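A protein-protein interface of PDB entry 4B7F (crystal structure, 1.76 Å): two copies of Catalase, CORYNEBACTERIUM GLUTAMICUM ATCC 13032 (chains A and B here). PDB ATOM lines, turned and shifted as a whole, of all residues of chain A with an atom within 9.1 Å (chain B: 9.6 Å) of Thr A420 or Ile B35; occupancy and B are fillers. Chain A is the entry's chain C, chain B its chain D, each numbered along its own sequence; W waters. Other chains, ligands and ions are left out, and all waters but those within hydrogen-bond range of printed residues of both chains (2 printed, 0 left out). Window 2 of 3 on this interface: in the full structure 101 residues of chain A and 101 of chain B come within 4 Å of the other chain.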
ATOM      1  N   SER A 398      -0.953  14.475  25.106  1.00  0.00           N
ATOM      2  CA  SER A 398      -2.013  15.039  24.280  1.00  0.00           C
ATOM      3  C   SER A 398      -1.873  14.497  22.855  1.00  0.00           C
ATOM      4  O   SER A 398      -0.757  14.238  22.386  1.00  0.00           O
ATOM      5  CB  SER A 398      -1.990  16.570  24.304  1.00  0.00           C
ATOM      6  OG  SER A 398      -1.228  17.096  23.237  1.00  0.00           O
ATOM      7  N   GLY A 407      -1.828  22.672  21.622  1.00  0.00           N
ATOM      8  CA  GLY A 407      -1.350  23.917  21.042  1.00  0.00           C
ATOM      9  C   GLY A 407      -2.496  24.805  20.594  1.00  0.00           C
ATOM     10  O   GLY A 407      -3.610  24.322  20.378  1.00  0.00           O
ATOM     11  N   LEU A 409      -2.834  26.060  17.792  1.00  0.00           N
ATOM     12  CA  LEU A 409      -3.131  25.725  16.397  1.00  0.00           C
ATOM     13  C   LEU A 409      -3.902  24.415  16.295  1.00  0.00           C
ATOM     14  O   LEU A 409      -4.599  24.171  15.298  1.00  0.00           O
ATOM     15  CB  LEU A 409      -1.852  25.613  15.558  1.00  0.00           C
ATOM     16  CG  LEU A 409      -0.995  26.869  15.378  1.00  0.00           C
ATOM     17  CD1 LEU A 409       0.223  26.573  14.507  1.00  0.00           C
ATOM     18  CD2 LEU A 409      -1.818  27.999  14.779  1.00  0.00           C
ATOM     19  N   ASP A 410      -3.764  23.571  17.317  1.00  0.00           N
ATOM     20  CA  ASP A 410      -4.450  22.279  17.358  1.00  0.00           C
ATOM     21  C   ASP A 410      -5.890  22.449  17.846  1.00  0.00           C
ATOM     22  O   ASP A 410      -6.251  23.493  18.402  1.00  0.00           O
ATOM     23  CB  ASP A 410      -3.729  21.306  18.307  1.00  0.00           C
ATOM     24  CG  ASP A 410      -2.223  21.237  18.075  1.00  0.00           C
ATOM     25  OD1 ASP A 410      -1.782  21.192  16.905  1.00  0.00           O
ATOM     26  OD2 ASP A 410      -1.486  21.220  19.085  1.00  0.00           O
ATOM     27  N   ASN A 411      -6.702  21.405  17.680  1.00  0.00           N
ATOM     28  CA  ASN A 411      -8.094  21.449  18.136  1.00  0.00           C
ATOM     29  C   ASN A 411      -8.297  20.903  19.540  1.00  0.00           C
ATOM     30  O   ASN A 411      -9.388  21.010  20.105  1.00  0.00           O
ATOM     31  CB  ASN A 411      -9.029  20.735  17.147  1.00  0.00           C
ATOM     32  CG  ASN A 411      -8.691  19.259  16.971  1.00  0.00           C
ATOM     33  OD1 ASN A 411      -8.045  18.646  17.824  1.00  0.00           O
ATOM     34  ND2 ASN A 411      -9.134  18.680  15.858  1.00  0.00           N
ATOM     35  N   ASP A 414      -7.539  15.794  18.753  1.00  0.00           N
ATOM     36  CA  ASP A 414      -6.855  14.794  17.931  1.00  0.00           C
ATOM     37  C   ASP A 414      -5.429  15.198  17.549  1.00  0.00           C
ATOM     38  O   ASP A 414      -4.946  16.271  17.943  1.00  0.00           O
ATOM     39  CB  ASP A 414      -7.670  14.437  16.677  1.00  0.00           C
ATOM     40  CG  ASP A 414      -7.907  15.629  15.767  1.00  0.00           C
ATOM     41  OD1 ASP A 414      -6.952  16.380  15.467  1.00  0.00           O
ATOM     42  OD2 ASP A 414      -9.068  15.818  15.344  1.00  0.00           O
ATOM     43  N   SER A 415      -4.780  14.339  16.768  1.00  0.00           N
ATOM     44  CA  SER A 415      -3.359  14.474  16.439  1.00  0.00           C
ATOM     45  C   SER A 415      -3.068  15.295  15.185  1.00  0.00           C
ATOM     46  O   SER A 415      -1.929  15.291  14.694  1.00  0.00           O
ATOM     47  CB  SER A 415      -2.754  13.092  16.239  1.00  0.00           C
ATOM     48  OG  SER A 415      -3.391  12.443  15.153  1.00  0.00           O
ATOM     49  N   SER A 416      -4.078  15.987  14.662  1.00  0.00           N
ATOM     50  CA  SER A 416      -3.908  16.764  13.441  1.00  0.00           C
ATOM     51  C   SER A 416      -3.474  15.900  12.266  1.00  0.00           C
ATOM     52  O   SER A 416      -2.663  16.321  11.435  1.00  0.00           O
ATOM     53  CB  SER A 416      -2.931  17.934  13.640  1.00  0.00           C
ATOM     54  OG  SER A 416      -3.426  18.837  14.613  1.00  0.00           O
ATOM     55  N   SER A 417      -4.022  14.691  12.183  1.00  0.00           N
ATOM     56  CA  SER A 417      -3.766  13.856  11.015  1.00  0.00           C
ATOM     57  C   SER A 417      -4.694  14.298   9.881  1.00  0.00           C
ATOM     58  O   SER A 417      -5.172  15.444   9.870  1.00  0.00           O
ATOM     59  CB  SER A 417      -3.963  12.373  11.347  1.00  0.00           C
ATOM     60  OG  SER A 417      -3.467  11.529  10.319  1.00  0.00           O
ATOM     61  N   ASN A 418      -4.954  13.385   8.949  1.00  0.00           N
ATOM     62  CA  ASN A 418      -5.764  13.679   7.765  1.00  0.00           C
ATOM     63  C   ASN A 418      -5.247  14.902   7.028  1.00  0.00           C
ATOM     64  O   ASN A 418      -6.028  15.758   6.598  1.00  0.00           O
ATOM     65  CB  ASN A 418      -7.238  13.854   8.138  1.00  0.00           C
ATOM     66  CG  ASN A 418      -7.794  12.649   8.853  1.00  0.00           C
ATOM     67  OD1 ASN A 418      -7.479  11.515   8.500  1.00  0.00           O
ATOM     68  ND2 ASN A 418      -8.609  12.884   9.878  1.00  0.00           N
ATOM     69  N   HIS A 419      -4.130  14.913   6.952  1.00  0.00           N
ATOM     70  CA  HIS A 419      -3.334  15.926   6.276  1.00  0.00           C
ATOM     71  C   HIS A 419      -3.652  17.357   6.684  1.00  0.00           C
ATOM     72  O   HIS A 419      -3.758  18.246   5.841  1.00  0.00           O
ATOM     73  CB  HIS A 419      -3.393  15.716   4.761  1.00  0.00           C
ATOM     74  CG  HIS A 419      -2.741  14.444   4.327  1.00  0.00           C
ATOM     75  ND1 HIS A 419      -3.388  13.226   4.361  1.00  0.00           N
ATOM     76  CD2 HIS A 419      -1.520  14.207   3.794  1.00  0.00           C
ATOM     77  CE1 HIS A 419      -2.585  12.291   3.890  1.00  0.00           C
ATOM     78  NE2 HIS A 419      -1.445  12.858   3.541  1.00  0.00           N
ATOM     79  N   THR A 420      -3.689  17.667   7.896  1.00  0.00           N
ATOM     80  CA  THR A 420      -3.900  18.995   8.457  1.00  0.00           C
ATOM     81  C   THR A 420      -2.626  19.815   8.290  1.00  0.00           C
ATOM     82  O   THR A 420      -1.542  19.345   8.643  1.00  0.00           O
ATOM     83  CB  THR A 420      -4.238  18.894   9.958  1.00  0.00           C
ATOM     84  OG1 THR A 420      -5.435  18.120  10.128  1.00  0.00           O
ATOM     85  CG2 THR A 420      -4.429  20.285  10.594  1.00  0.00           C
ATOM     86  N   SER A 421      -2.747  21.024   7.738  1.00  0.00           N
ATOM     87  CA  SER A 421      -1.612  21.949   7.658  1.00  0.00           C
ATOM     88  C   SER A 421      -1.958  23.269   8.337  1.00  0.00           C
ATOM     89  O   SER A 421      -3.120  23.694   8.318  1.00  0.00           O
ATOM     90  CB  SER A 421      -1.194  22.190   6.207  1.00  0.00           C
ATOM     91  OG  SER A 421      -0.641  21.024   5.628  1.00  0.00           O
ATOM     92  N   TYR A 422      -0.950  23.914   8.932  1.00  0.00           N
ATOM     93  CA  TYR A 422      -1.146  25.163   9.664  1.00  0.00           C
ATOM     94  C   TYR A 422      -0.536  26.375   8.948  1.00  0.00           C
ATOM     95  O   TYR A 422      -0.874  27.515   9.259  1.00  0.00           O
ATOM     96  CB  TYR A 422      -0.528  25.067  11.053  1.00  0.00           C
ATOM     97  CG  TYR A 422      -1.153  24.050  11.980  1.00  0.00           C
ATOM     98  CD1 TYR A 422      -2.516  23.783  11.945  1.00  0.00           C
ATOM     99  CD2 TYR A 422      -0.373  23.366  12.903  1.00  0.00           C
ATOM    100  CE1 TYR A 422      -3.085  22.857  12.811  1.00  0.00           C
ATOM    101  CE2 TYR A 422      -0.931  22.441  13.772  1.00  0.00           C
ATOM    102  CZ  TYR A 422      -2.280  22.188  13.719  1.00  0.00           C
ATOM    103  OH  TYR A 422      -2.824  21.267  14.587  1.00  0.00           O
ATOM    104  N   GLY A 423       0.375  26.134   8.009  1.00  0.00           N
ATOM    105  CA  GLY A 423       0.992  27.228   7.270  1.00  0.00           C
ATOM    106  C   GLY A 423       2.231  27.833   7.915  1.00  0.00           C
ATOM    107  O   GLY A 423       2.896  27.203   8.738  1.00  0.00           O
ATOM    108  N   ALA A 425       5.151  29.440   9.906  1.00  0.00           N
ATOM    109  CA  ALA A 425       5.459  29.494  11.335  1.00  0.00           C
ATOM    110  C   ALA A 425       5.969  30.863  11.747  1.00  0.00           C
ATOM    111  O   ALA A 425       7.156  31.025  12.074  1.00  0.00           O
ATOM    112  CB  ALA A 425       6.477  28.416  11.698  1.00  0.00           C
ATOM    113  N   ASP A 427       5.515  32.543  14.370  1.00  0.00           N
ATOM    114  CA  ASP A 427       5.954  32.586  15.767  1.00  0.00           C
ATOM    115  C   ASP A 427       7.448  32.279  15.919  1.00  0.00           C
ATOM    116  O   ASP A 427       8.046  32.554  16.970  1.00  0.00           O
ATOM    117  CB  ASP A 427       5.167  31.565  16.579  1.00  0.00           C
ATOM    118  CG  ASP A 427       5.309  30.177  16.019  1.00  0.00           C
ATOM    119  OD1 ASP A 427       4.671  29.902  14.985  1.00  0.00           O
ATOM    120  OD2 ASP A 427       6.053  29.356  16.607  1.00  0.00           O
ATOM    121  N   ILE A 428       8.030  31.672  14.888  1.00  0.00           N
ATOM    122  CA  ILE A 428       9.472  31.480  14.818  1.00  0.00           C
ATOM    123  C   ILE A 428      10.048  32.709  14.109  1.00  0.00           C
ATOM    124  O   ILE A 428      10.785  33.492  14.718  1.00  0.00           O
ATOM    125  CB  ILE A 428       9.821  30.159  14.103  1.00  0.00           C
ATOM    126  CG1 ILE A 428       9.205  28.982  14.864  1.00  0.00           C
ATOM    127  CG2 ILE A 428      11.331  29.960  13.994  1.00  0.00           C
ATOM    128  CD1 ILE A 428       9.495  27.626  14.237  1.00  0.00           C
ATOM    129  N   VAL B  30       2.163  27.628  23.130  1.00  0.00           N
ATOM    130  CA  VAL B  30       2.633  26.593  22.212  1.00  0.00           C
ATOM    131  C   VAL B  30       1.720  26.566  20.992  1.00  0.00           C
ATOM    132  O   VAL B  30       0.496  26.467  21.144  1.00  0.00           O
ATOM    133  CB  VAL B  30       2.577  25.210  22.907  1.00  0.00           C
ATOM    134  CG1 VAL B  30       2.694  24.084  21.903  1.00  0.00           C
ATOM    135  CG2 VAL B  30       3.661  25.108  23.969  1.00  0.00           C
ATOM    136  N   PRO B  31       2.295  26.659  19.779  1.00  0.00           N
ATOM    137  CA  PRO B  31       1.443  26.594  18.584  1.00  0.00           C
ATOM    138  C   PRO B  31       0.891  25.192  18.360  1.00  0.00           C
ATOM    139  O   PRO B  31      -0.311  25.029  18.098  1.00  0.00           O
ATOM    140  CB  PRO B  31       2.401  26.966  17.439  1.00  0.00           C
ATOM    141  CG  PRO B  31       3.579  27.646  18.117  1.00  0.00           C
ATOM    142  CD  PRO B  31       3.699  26.943  19.436  1.00  0.00           C
ATOM    143  N   SER B  32       1.756  24.185  18.449  1.00  0.00           N
ATOM    144  CA  SER B  32       1.303  22.817  18.229  1.00  0.00           C
ATOM    145  C   SER B  32       1.989  21.756  19.084  1.00  0.00           C
ATOM    146  O   SER B  32       3.202  21.812  19.311  1.00  0.00           O
ATOM    147  CB  SER B  32       1.481  22.434  16.766  1.00  0.00           C
ATOM    148  OG  SER B  32       0.896  21.167  16.530  1.00  0.00           O
ATOM    149  N   GLU B  33       1.208  20.768  19.517  1.00  0.00           N
ATOM    150  CA  GLU B  33       1.758  19.579  20.169  1.00  0.00           C
ATOM    151  C   GLU B  33       1.780  18.426  19.169  1.00  0.00           C
ATOM    152  O   GLU B  33       2.104  17.285  19.526  1.00  0.00           O
ATOM    153  CB  GLU B  33       0.893  19.161  21.370  1.00  0.00           C
ATOM    154  CG  GLU B  33       0.777  20.181  22.509  1.00  0.00           C
ATOM    155  CD  GLU B  33       2.062  20.344  23.304  1.00  0.00           C
ATOM    156  OE1 GLU B  33       3.083  19.719  22.935  1.00  0.00           O
ATOM    157  OE2 GLU B  33       2.051  21.103  24.306  1.00  0.00           O
ATOM    158  N   ASN B  34       1.420  18.722  17.924  1.00  0.00           N
ATOM    159  CA  ASN B  34       1.196  17.692  16.914  1.00  0.00           C
ATOM    160  C   ASN B  34       2.151  17.706  15.734  1.00  0.00           C
ATOM    161  O   ASN B  34       2.529  16.655  15.228  1.00  0.00           O
ATOM    162  CB  ASN B  34      -0.238  17.786  16.368  1.00  0.00           C
ATOM    163  CG  ASN B  34      -1.284  17.415  17.398  1.00  0.00           C
ATOM    164  OD1 ASN B  34      -0.988  16.751  18.400  1.00  0.00           O
ATOM    165  ND2 ASN B  34      -2.525  17.848  17.160  1.00  0.00           N
ATOM    166  N   ILE B  35       2.509  18.897  15.264  1.00  0.00           N
ATOM    167  CA  ILE B  35       3.318  19.021  14.063  1.00  0.00           C
ATOM    168  C   ILE B  35       4.552  19.897  14.321  1.00  0.00           C
ATOM    169  O   ILE B  35       4.443  20.981  14.916  1.00  0.00           O
ATOM    170  CB  ILE B  35       2.500  19.640  12.914  1.00  0.00           C
ATOM    171  CG1 ILE B  35       1.164  18.911  12.750  1.00  0.00           C
ATOM    172  CG2 ILE B  35       3.281  19.607  11.614  1.00  0.00           C
ATOM    173  CD1 ILE B  35       0.261  19.541  11.677  1.00  0.00           C
ATOM    174  N   SER B  36       5.715  19.426  13.879  1.00  0.00           N
ATOM    175  CA  SER B  36       6.961  20.170  14.060  1.00  0.00           C
ATOM    176  C   SER B  36       7.220  21.052  12.840  1.00  0.00           C
ATOM    177  O   SER B  36       6.668  20.816  11.766  1.00  0.00           O
ATOM    178  CB  SER B  36       8.134  19.224  14.337  1.00  0.00           C
ATOM    179  OG  SER B  36       8.299  18.245  13.330  1.00  0.00           O
ATOM    180  N   ALA B  37       8.031  22.092  12.997  1.00  0.00           N
ATOM    181  CA  ALA B  37       8.214  23.029  11.892  1.00  0.00           C
ATOM    182  C   ALA B  37       9.321  22.579  10.945  1.00  0.00           C
ATOM    183  O   ALA B  37      10.404  22.174  11.379  1.00  0.00           O
ATOM    184  CB  ALA B  37       8.485  24.434  12.412  1.00  0.00           C
ATOM    185  N   THR B  38       9.044  22.658   9.644  1.00  0.00           N
ATOM    186  CA  THR B  38       9.993  22.241   8.621  1.00  0.00           C
ATOM    187  C   THR B  38      10.179  23.334   7.573  1.00  0.00           C
ATOM    188  O   THR B  38       9.349  24.245   7.442  1.00  0.00           O
ATOM    189  CB  THR B  38       9.510  20.966   7.899  1.00  0.00           C
ATOM    190  OG1 THR B  38       8.157  21.161   7.471  1.00  0.00           O
ATOM    191  CG2 THR B  38       9.565  19.765   8.823  1.00  0.00           C
ATOM    192  N   GLY B  40       9.643  24.018   4.338  1.00  0.00           N
ATOM    193  CA  GLY B  40       8.855  23.417   3.272  1.00  0.00           C
ATOM    194  C   GLY B  40       8.253  22.142   3.841  1.00  0.00           C
ATOM    195  O   GLY B  40       8.882  21.497   4.678  1.00  0.00           O
ATOM    196  N   PRO B  41       7.027  21.788   3.416  1.00  0.00           N
ATOM    197  CA  PRO B  41       6.329  20.599   3.928  1.00  0.00           C
ATOM    198  C   PRO B  41       7.173  19.323   3.860  1.00  0.00           C
ATOM    199  O   PRO B  41       7.076  18.486   4.763  1.00  0.00           O
ATOM    200  CB  PRO B  41       5.124  20.476   2.989  1.00  0.00           C
ATOM    201  CG  PRO B  41       4.852  21.873   2.553  1.00  0.00           C
ATOM    202  CD  PRO B  41       6.205  22.544   2.453  1.00  0.00           C
ATOM    203  N   ASN B  45      13.543  19.321   9.097  1.00  0.00           N
ATOM    204  CA  ASN B  45      13.173  19.968  10.343  1.00  0.00           C
ATOM    205  C   ASN B  45      14.145  21.097  10.654  1.00  0.00           C
ATOM    206  O   ASN B  45      15.355  20.951  10.474  1.00  0.00           O
ATOM    207  CB  ASN B  45      13.163  18.965  11.485  1.00  0.00           C
ATOM    208  CG  ASN B  45      11.882  18.184  11.537  1.00  0.00           C
ATOM    209  OD1 ASN B  45      10.961  18.528  12.286  1.00  0.00           O
ATOM    210  ND2 ASN B  45      11.791  17.145  10.711  1.00  0.00           N
ATOM    211  N   VAL B  46      13.614  22.220  11.124  1.00  0.00           N
ATOM    212  CA  VAL B  46      14.466  23.360  11.450  1.00  0.00           C
ATOM    213  C   VAL B  46      14.964  23.233  12.880  1.00  0.00           C
ATOM    214  O   VAL B  46      14.290  22.647  13.732  1.00  0.00           O
ATOM    215  CB  VAL B  46      13.727  24.709  11.251  1.00  0.00           C
ATOM    216  CG1 VAL B  46      13.166  24.794   9.838  1.00  0.00           C
ATOM    217  CG2 VAL B  46      12.602  24.876  12.279  1.00  0.00           C
ATOM    218  N   ASP B  49      12.665  25.047  16.049  1.00  0.00           N
ATOM    219  CA  ASP B  49      11.381  24.708  16.633  1.00  0.00           C
ATOM    220  C   ASP B  49      11.676  24.565  18.123  1.00  0.00           C
ATOM    221  O   ASP B  49      12.013  23.479  18.603  1.00  0.00           O
ATOM    222  CB  ASP B  49      10.801  23.418  16.049  1.00  0.00           C
ATOM    223  CG  ASP B  49       9.358  23.197  16.449  1.00  0.00           C
ATOM    224  OD1 ASP B  49       8.978  23.626  17.558  1.00  0.00           O
ATOM    225  OD2 ASP B  49       8.597  22.597  15.654  1.00  0.00           O
ATOM    226  N   ILE B  50      11.573  25.687  18.833  1.00  0.00           N
ATOM    227  CA  ILE B  50      11.963  25.775  20.231  1.00  0.00           C
ATOM    228  C   ILE B  50      11.179  24.783  21.080  1.00  0.00           C
ATOM    229  O   ILE B  50      11.766  24.071  21.901  1.00  0.00           O
ATOM    230  CB  ILE B  50      11.764  27.202  20.761  1.00  0.00           C
ATOM    231  CG1 ILE B  50      12.572  28.186  19.912  1.00  0.00           C
ATOM    232  CG2 ILE B  50      12.188  27.299  22.229  1.00  0.00           C
ATOM    233  CD1 ILE B  50      12.242  29.666  20.178  1.00  0.00           C
ATOM    234  N   HIS B  51       9.864  24.721  20.869  1.00  0.00           N
ATOM    235  CA  HIS B  51       9.018  23.818  21.653  1.00  0.00           C
ATOM    236  C   HIS B  51       9.389  22.358  21.420  1.00  0.00           C
ATOM    237  O   HIS B  51       9.449  21.582  22.374  1.00  0.00           O
ATOM    238  CB  HIS B  51       7.529  24.038  21.356  1.00  0.00           C
ATOM    239  CG  HIS B  51       6.629  23.072  22.059  1.00  0.00           C
ATOM    240  ND1 HIS B  51       6.578  22.963  23.435  1.00  0.00           N
ATOM    241  CD2 HIS B  51       5.737  22.167  21.583  1.00  0.00           C
ATOM    242  CE1 HIS B  51       5.701  22.030  23.769  1.00  0.00           C
ATOM    243  NE2 HIS B  51       5.181  21.532  22.666  1.00  0.00           N
ATOM    244  N   LEU B  52       9.631  21.981  20.161  1.00  0.00           N
ATOM    245  CA  LEU B  52      10.044  20.608  19.858  1.00  0.00           C
ATOM    246  C   LEU B  52      11.270  20.203  20.674  1.00  0.00           C
ATOM    247  O   LEU B  52      11.283  19.157  21.334  1.00  0.00           O
ATOM    248  CB  LEU B  52      10.338  20.433  18.354  1.00  0.00           C
ATOM    249  CG  LEU B  52      10.860  19.056  17.917  1.00  0.00           C
ATOM    250  CD1 LEU B  52       9.783  17.966  18.132  1.00  0.00           C
ATOM    251  CD2 LEU B  52      11.378  19.026  16.468  1.00  0.00           C
ATOM    252  N   LYS B  55      10.588  20.058  24.429  1.00  0.00           N
ATOM    253  CA  LYS B  55       9.753  18.899  24.735  1.00  0.00           C
ATOM    254  C   LYS B  55      10.577  17.605  24.704  1.00  0.00           C
ATOM    255  O   LYS B  55      10.490  16.775  25.616  1.00  0.00           O
ATOM    256  CB  LYS B  55       8.607  18.817  23.730  1.00  0.00           C
ATOM    257  CG  LYS B  55       7.517  17.790  24.081  1.00  0.00           C
ATOM    258  CD  LYS B  55       6.403  17.879  23.015  1.00  0.00           C
ATOM    259  CE  LYS B  55       5.201  17.005  23.378  1.00  0.00           C
ATOM    260  NZ  LYS B  55       4.062  17.220  22.420  1.00  0.00           N
HETATM  261  O   HOH W   1       1.349  17.256  24.192  1.00  0.00           O
HETATM  262  O   HOH W   2      -2.582  17.235  20.765  1.00  0.00           O
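The backbone carbonyl oxygen of Pro B31 sits at hydrogen-bond distance from the backbone NH of Leu A409, 2.7 Å away. The side-chain hydroxyl of Ser B32 lies within hydrogen-bond range of the side-chain carboxylate of Asp A410 (2.7 Å). N of Glu B33 sits at hydrogen-bond distance from OD2 of Asp A410 (2.8 Å). The side-chain carboxylate (OD1) of Asp A410 is in hydrogen-bond range of the side-chain amide nitrogen (ND2) of Asn B34. The side-chain amide nitrogen (ND2) of Asn B34 lies within hydrogen-bond range of the backbone carbonyl oxygen (O) of Asp A414, 3.0 Å away. OG of Ser A416 is in hydrogen-bond range of ND2 of Asn B34.
N of Gly A407 is in hydrogen-bond range of OD2 of Asp A410. The side-chain carboxylate (OD1) of Asp A414 sits at hydrogen-bond distance from the backbone NH (N) of Ser A416, 3.0 Å away. The side-chain hydroxyl (OG) of Ser B32 sits at hydrogen-bond distance from the backbone NH (N) of Asn B34 (2.9 Å). OG of Ser B32 is in hydrogen-bond range of N of Ile B35 (3.1 Å). OE1 of Glu B33 sits at hydrogen-bond distance from NE2 of His B51. The side-chain carboxylate (OE1) of Glu B33 lies within salt-bridge range of the side-chain amino group (NZ) of Lys B55 (2.7 Å).
Among the printed residues, merely in contact across the chains: Ser A398 with Glu B33 (3.5 Å), Gly A407 with Val B30 (3.1 Å), Gly A407 with Pro B31 (3.3 Å), Gly A407 with Glu B33 (3.7 Å), Asp A410 with Pro B31 (3.8 Å), Ser A415 with Asn B34 (3.3 Å), Thr A420 with Ile B35 (3.5 Å), Tyr A422 with Ser B32 (3.5 Å), Tyr A422 with Ile B35 (3.8 Å), Asp A427 with Pro B31 (3.4 Å) and Ile A428 with Ala B37 (3.8 Å).
Of the printed residues of chain B, Ser A398 touches Glu B33 (3.5 Å). Of the printed residues of chain B, Gly A407 touches Val B30, Pro B31 and Glu B33. Printed residues of chain B within 4 Å of Ser A415: Asn B34 (3.3 Å). Ser A416 touches one residue of chain B. Of chain B, only Ile B35 comes within 4 Å of Thr A420. Ser A421 touches none of the printed residues of chain B. Of the printed residues of chain B, Asp A427 touches Pro B31 (3.4 Å). Printed residues of chain A within 4 Å of Ser B32: Asp A410 (2.7 Å) and Tyr A422 (3.5 Å). Ile B35 touches just these residues of chain A: Thr A420 (3.5 Å) and Tyr A422 (3.8 Å). No residue of chain A comes within 4 Å of Ser B36. Gly B40 touches none of the printed residues of chain A. The nearest residue of chain A that does not touch Ile B35 is Ser A416 (4.1 Å). The nearest printed residue of chain B that does not touch Gly A407 is Ser B32 (4.02 Å).
Printed residues of chain B that touch a printed residue of chain A: Val B30, Pro B31, Ser B32, Glu B33, Asn B34, Ile B35 and Ala B37. Of the 18 printed residues of chain A, 11 touch a printed residue of chain B. Hydrophobic or aromatic side chains of chain A that line the printed part of chain B: Leu A409, Tyr A422 and Ile A428. Among the printed residues, 17 pairs touch across the chains. Among the printed residues, no Asp or Glu carboxylate lies within 4 Å of a Lys or Arg side-chain nitrogen of the other chain.
No position is printed for both chains. Of the 17 pairs that touch across the chains among the printed residues, none has its exchanged pair printed and touching as well.
Water W1 lies within hydrogen-bond range of OG of Ser A398, NZ of Lys B55 and OE1 of Glu B33. Water W2 lies within hydrogen-bond range of OG of Ser A398 and OD1 of Asn B34.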
